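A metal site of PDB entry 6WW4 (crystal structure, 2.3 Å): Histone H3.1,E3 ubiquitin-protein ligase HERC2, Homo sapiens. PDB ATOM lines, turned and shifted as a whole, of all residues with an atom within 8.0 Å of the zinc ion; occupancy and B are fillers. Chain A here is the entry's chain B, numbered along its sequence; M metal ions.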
ATOM      1  N   THR A  12     -12.618  -7.634  -7.820  1.00  0.00           N
ATOM      2  CA  THR A  12     -12.526  -6.689  -6.720  1.00  0.00           C
ATOM      3  C   THR A  12     -12.412  -7.465  -5.416  1.00  0.00           C
ATOM      4  O   THR A  12     -13.135  -8.443  -5.224  1.00  0.00           O
ATOM      5  CB  THR A  12     -13.756  -5.773  -6.674  1.00  0.00           C
ATOM      6  OG1 THR A  12     -13.956  -5.155  -7.951  1.00  0.00           O
ATOM      7  CG2 THR A  12     -13.605  -4.695  -5.606  1.00  0.00           C
ATOM      8  N   CYS A  13     -11.510  -7.035  -4.538  1.00  0.00           N
ATOM      9  CA  CYS A  13     -11.487  -7.577  -3.188  1.00  0.00           C
ATOM     10  C   CYS A  13     -12.697  -7.094  -2.415  1.00  0.00           C
ATOM     11  O   CYS A  13     -12.951  -5.887  -2.336  1.00  0.00           O
ATOM     12  CB  CYS A  13     -10.206  -7.176  -2.448  1.00  0.00           C
ATOM     13  SG  CYS A  13     -10.194  -7.740  -0.697  1.00  0.00           S
ATOM     14  N   ASP A  14     -13.458  -8.033  -1.854  1.00  0.00           N
ATOM     15  CA  ASP A  14     -14.638  -7.668  -1.088  1.00  0.00           C
ATOM     16  C   ASP A  14     -14.289  -7.133   0.286  1.00  0.00           C
ATOM     17  O   ASP A  14     -15.144  -6.508   0.926  1.00  0.00           O
ATOM     18  CB  ASP A  14     -15.576  -8.866  -0.948  1.00  0.00           C
ATOM     19  CG  ASP A  14     -16.360  -9.125  -2.226  1.00  0.00           C
ATOM     20  OD1 ASP A  14     -15.983 -10.052  -2.987  1.00  0.00           O
ATOM     21  OD2 ASP A  14     -17.333  -8.391  -2.468  1.00  0.00           O
ATOM     22  N   GLY A  15     -13.062  -7.359   0.738  1.00  0.00           N
ATOM     23  CA  GLY A  15     -12.629  -6.896   2.042  1.00  0.00           C
ATOM     24  C   GLY A  15     -12.078  -5.483   2.023  1.00  0.00           C
ATOM     25  O   GLY A  15     -12.304  -4.722   2.963  1.00  0.00           O
ATOM     26  N   CYS A  16     -11.377  -5.100   0.965  1.00  0.00           N
ATOM     27  CA  CYS A  16     -10.753  -3.787   0.917  1.00  0.00           C
ATOM     28  C   CYS A  16     -11.017  -3.002  -0.357  1.00  0.00           C
ATOM     29  O   CYS A  16     -10.489  -1.894  -0.497  1.00  0.00           O
ATOM     30  CB  CYS A  16      -9.229  -3.919   1.124  1.00  0.00           C
ATOM     31  SG  CYS A  16      -8.400  -4.607  -0.309  1.00  0.00           S
ATOM     32  N   GLN A  17     -11.812  -3.528  -1.286  1.00  0.00           N
ATOM     33  CA  GLN A  17     -12.171  -2.871  -2.537  1.00  0.00           C
ATOM     34  C   GLN A  17     -10.968  -2.619  -3.434  1.00  0.00           C
ATOM     35  O   GLN A  17     -11.030  -1.769  -4.326  1.00  0.00           O
ATOM     36  CB  GLN A  17     -12.936  -1.571  -2.289  1.00  0.00           C
ATOM     37  CG  GLN A  17     -13.958  -1.692  -1.142  1.00  0.00           C
ATOM     38  CD  GLN A  17     -15.300  -1.128  -1.496  1.00  0.00           C
ATOM     39  OE1 GLN A  17     -16.125  -1.789  -2.120  1.00  0.00           O
ATOM     40  NE2 GLN A  17     -15.542   0.114  -1.098  1.00  0.00           N
ATOM     41  N   MET A  18      -9.875  -3.341  -3.216  1.00  0.00           N
ATOM     42  CA  MET A  18      -8.816  -3.392  -4.201  1.00  0.00           C
ATOM     43  C   MET A  18      -9.374  -3.803  -5.566  1.00  0.00           C
ATOM     44  O   MET A  18     -10.083  -4.799  -5.684  1.00  0.00           O
ATOM     45  CB  MET A  18      -7.722  -4.363  -3.762  1.00  0.00           C
ATOM     46  CG  MET A  18      -6.594  -4.481  -4.772  1.00  0.00           C
ATOM     47  SD  MET A  18      -5.284  -5.652  -4.343  1.00  0.00           S
ATOM     48  CE  MET A  18      -3.945  -4.922  -5.285  1.00  0.00           C
ATOM     49  N   PHE A  19      -9.033  -3.029  -6.584  1.00  0.00           N
ATOM     50  CA  PHE A  19      -9.464  -3.341  -7.944  1.00  0.00           C
ATOM     51  C   PHE A  19      -8.568  -2.752  -9.013  1.00  0.00           C
ATOM     52  O   PHE A  19      -8.411  -1.540  -9.105  1.00  0.00           O
ATOM     53  CB  PHE A  19     -10.884  -2.863  -8.194  1.00  0.00           C
ATOM     54  CG  PHE A  19     -11.327  -3.045  -9.603  1.00  0.00           C
ATOM     55  CD1 PHE A  19     -11.739  -4.279 -10.054  1.00  0.00           C
ATOM     56  CD2 PHE A  19     -11.301  -1.987 -10.502  1.00  0.00           C
ATOM     57  CE1 PHE A  19     -12.139  -4.456 -11.374  1.00  0.00           C
ATOM     58  CE2 PHE A  19     -11.688  -2.157 -11.809  1.00  0.00           C
ATOM     59  CZ  PHE A  19     -12.114  -3.397 -12.243  1.00  0.00           C
ATOM     60  N   ILE A  21      -7.637  -6.893  -8.244  1.00  0.00           N
ATOM     61  CA  ILE A  21      -6.759  -7.564  -7.297  1.00  0.00           C
ATOM     62  C   ILE A  21      -5.422  -7.864  -7.954  1.00  0.00           C
ATOM     63  O   ILE A  21      -5.348  -8.431  -9.054  1.00  0.00           O
ATOM     64  CB  ILE A  21      -7.412  -8.861  -6.773  1.00  0.00           C
ATOM     65  CG1 ILE A  21      -8.601  -8.537  -5.857  1.00  0.00           C
ATOM     66  CG2 ILE A  21      -6.385  -9.700  -6.023  1.00  0.00           C
ATOM     67  CD1 ILE A  21      -9.231  -9.749  -5.197  1.00  0.00           C
ATOM     68  N   ASP A  35     -14.439 -12.554  -3.105  1.00  0.00           N
ATOM     69  CA  ASP A  35     -13.003 -12.671  -3.299  1.00  0.00           C
ATOM     70  C   ASP A  35     -12.241 -11.837  -2.282  1.00  0.00           C
ATOM     71  O   ASP A  35     -12.687 -10.775  -1.860  1.00  0.00           O
ATOM     72  CB  ASP A  35     -12.576 -12.242  -4.714  1.00  0.00           C
ATOM     73  CG  ASP A  35     -13.156 -13.121  -5.808  1.00  0.00           C
ATOM     74  OD1 ASP A  35     -14.205 -12.752  -6.376  1.00  0.00           O
ATOM     75  OD2 ASP A  35     -12.554 -14.181  -6.090  1.00  0.00           O
ATOM     76  N   PHE A  36     -11.069 -12.331  -1.905  1.00  0.00           N
ATOM     77  CA  PHE A  36     -10.118 -11.637  -1.048  1.00  0.00           C
ATOM     78  C   PHE A  36      -8.786 -11.481  -1.747  1.00  0.00           C
ATOM     79  O   PHE A  36      -8.295 -12.411  -2.398  1.00  0.00           O
ATOM     80  CB  PHE A  36      -9.878 -12.398   0.268  1.00  0.00           C
ATOM     81  CG  PHE A  36     -10.791 -11.980   1.369  1.00  0.00           C
ATOM     82  CD1 PHE A  36     -11.551 -10.834   1.260  1.00  0.00           C
ATOM     83  CD2 PHE A  36     -10.890 -12.749   2.513  1.00  0.00           C
ATOM     84  CE1 PHE A  36     -12.391 -10.440   2.281  1.00  0.00           C
ATOM     85  CE2 PHE A  36     -11.743 -12.370   3.525  1.00  0.00           C
ATOM     86  CZ  PHE A  36     -12.490 -11.214   3.412  1.00  0.00           C
ATOM     87  N   CYS A  37      -8.185 -10.307  -1.615  1.00  0.00           N
ATOM     88  CA  CYS A  37      -6.754 -10.203  -1.846  1.00  0.00           C
ATOM     89  C   CYS A  37      -6.017 -10.958  -0.744  1.00  0.00           C
ATOM     90  O   CYS A  37      -6.613 -11.413   0.239  1.00  0.00           O
ATOM     91  CB  CYS A  37      -6.342  -8.739  -1.896  1.00  0.00           C
ATOM     92  SG  CYS A  37      -6.308  -7.932  -0.294  1.00  0.00           S
ATOM     93  N   GLU A  38      -4.704 -11.123  -0.893  1.00  0.00           N
ATOM     94  CA  GLU A  38      -4.011 -11.961   0.081  1.00  0.00           C
ATOM     95  C   GLU A  38      -4.027 -11.316   1.463  1.00  0.00           C
ATOM     96  O   GLU A  38      -4.227 -12.004   2.475  1.00  0.00           O
ATOM     97  CB  GLU A  38      -2.576 -12.238  -0.340  1.00  0.00           C
ATOM     98  CG  GLU A  38      -1.966 -13.340   0.495  1.00  0.00           C
ATOM     99  CD  GLU A  38      -0.476 -13.423   0.351  1.00  0.00           C
ATOM    100  OE1 GLU A  38       0.203 -13.603   1.396  1.00  0.00           O
ATOM    101  OE2 GLU A  38       0.022 -13.310  -0.779  1.00  0.00           O
ATOM    102  N   THR A  39      -3.771 -10.014   1.529  1.00  0.00           N
ATOM    103  CA  THR A  39      -3.775  -9.351   2.814  1.00  0.00           C
ATOM    104  C   THR A  39      -5.111  -9.547   3.520  1.00  0.00           C
ATOM    105  O   THR A  39      -5.145  -9.853   4.713  1.00  0.00           O
ATOM    106  CB  THR A  39      -3.444  -7.865   2.641  1.00  0.00           C
ATOM    107  OG1 THR A  39      -2.128  -7.754   2.057  1.00  0.00           O
ATOM    108  CG2 THR A  39      -3.452  -7.154   3.968  1.00  0.00           C
ATOM    109  N   CYS A  40      -6.219  -9.406   2.786  1.00  0.00           N
ATOM    110  CA  CYS A  40      -7.528  -9.596   3.415  1.00  0.00           C
ATOM    111  C   CYS A  40      -7.746 -11.068   3.798  1.00  0.00           C
ATOM    112  O   CYS A  40      -8.314 -11.355   4.854  1.00  0.00           O
ATOM    113  CB  CYS A  40      -8.638  -9.108   2.491  1.00  0.00           C
ATOM    114  SG  CYS A  40      -8.767  -7.300   2.343  1.00  0.00           S
ATOM    115  N   PHE A  41      -7.298 -12.005   2.967  1.00  0.00           N
ATOM    116  CA  PHE A  41      -7.502 -13.403   3.316  1.00  0.00           C
ATOM    117  C   PHE A  41      -6.772 -13.752   4.614  1.00  0.00           C
ATOM    118  O   PHE A  41      -7.266 -14.572   5.403  1.00  0.00           O
ATOM    119  CB  PHE A  41      -7.055 -14.340   2.198  1.00  0.00           C
ATOM    120  CG  PHE A  41      -7.048 -15.787   2.624  1.00  0.00           C
ATOM    121  CD1 PHE A  41      -5.862 -16.433   2.967  1.00  0.00           C
ATOM    122  CD2 PHE A  41      -8.242 -16.502   2.742  1.00  0.00           C
ATOM    123  CE1 PHE A  41      -5.866 -17.767   3.380  1.00  0.00           C
ATOM    124  CE2 PHE A  41      -8.252 -17.835   3.162  1.00  0.00           C
ATOM    125  CZ  PHE A  41      -7.061 -18.459   3.475  1.00  0.00           C
ATOM    126  N   THR A  43      -6.110 -11.563   6.982  1.00  0.00           N
ATOM    127  CA  THR A  43      -6.434 -10.498   7.927  1.00  0.00           C
ATOM    128  C   THR A  43      -7.906 -10.451   8.342  1.00  0.00           C
ATOM    129  O   THR A  43      -8.202 -10.111   9.490  1.00  0.00           O
ATOM    130  CB  THR A  43      -6.020  -9.160   7.282  1.00  0.00           C
ATOM    131  OG1 THR A  43      -4.611  -8.956   7.466  1.00  0.00           O
ATOM    132  CG2 THR A  43      -6.787  -7.991   7.866  1.00  0.00           C
ATOM    133  N   LYS A  44      -8.838 -10.787   7.466  1.00  0.00           N
ATOM    134  CA  LYS A  44     -10.253 -10.586   7.735  1.00  0.00           C
ATOM    135  C   LYS A  44     -10.952 -11.919   7.886  1.00  0.00           C
ATOM    136  O   LYS A  44     -10.630 -12.883   7.182  1.00  0.00           O
ATOM    137  CB  LYS A  44     -10.889  -9.764   6.618  1.00  0.00           C
ATOM    138  CG  LYS A  44     -10.316  -8.357   6.548  1.00  0.00           C
ATOM    139  CD  LYS A  44     -11.085  -7.459   5.610  1.00  0.00           C
ATOM    140  CE  LYS A  44     -10.394  -6.114   5.462  1.00  0.00           C
ATOM    141  NZ  LYS A  44     -10.487  -5.323   6.735  1.00  0.00           N
HETATM  142 ZN    ZN M   1      -8.350  -6.878   0.198  1.00  0.00          ZN
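The side-chain sulfur (SG) of Cys 13 lies close to the backbone NH (N) of Gly 15 (3.2 Å). N of Cys 13 is in hydrogen-bond range of O of Met 18 (2.9 Å). SG of Cys 16 sits close to N of Met 18, 3.5 Å away. The side-chain sulfur (SG) of Cys 37 lies close to the backbone NH (N) of Thr 39.
Four residues have an atom within 4 Å of the zinc ion: Cys 13, Cys 16, Cys 37 and Cys 40.
The zinc ion is bound by SG of Cys 13 (2.2 Å), SG of Cys 40 (2.2 Å), SG of Cys 16 (2.3 Å) and SG of Cys 37 (2.4 Å).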
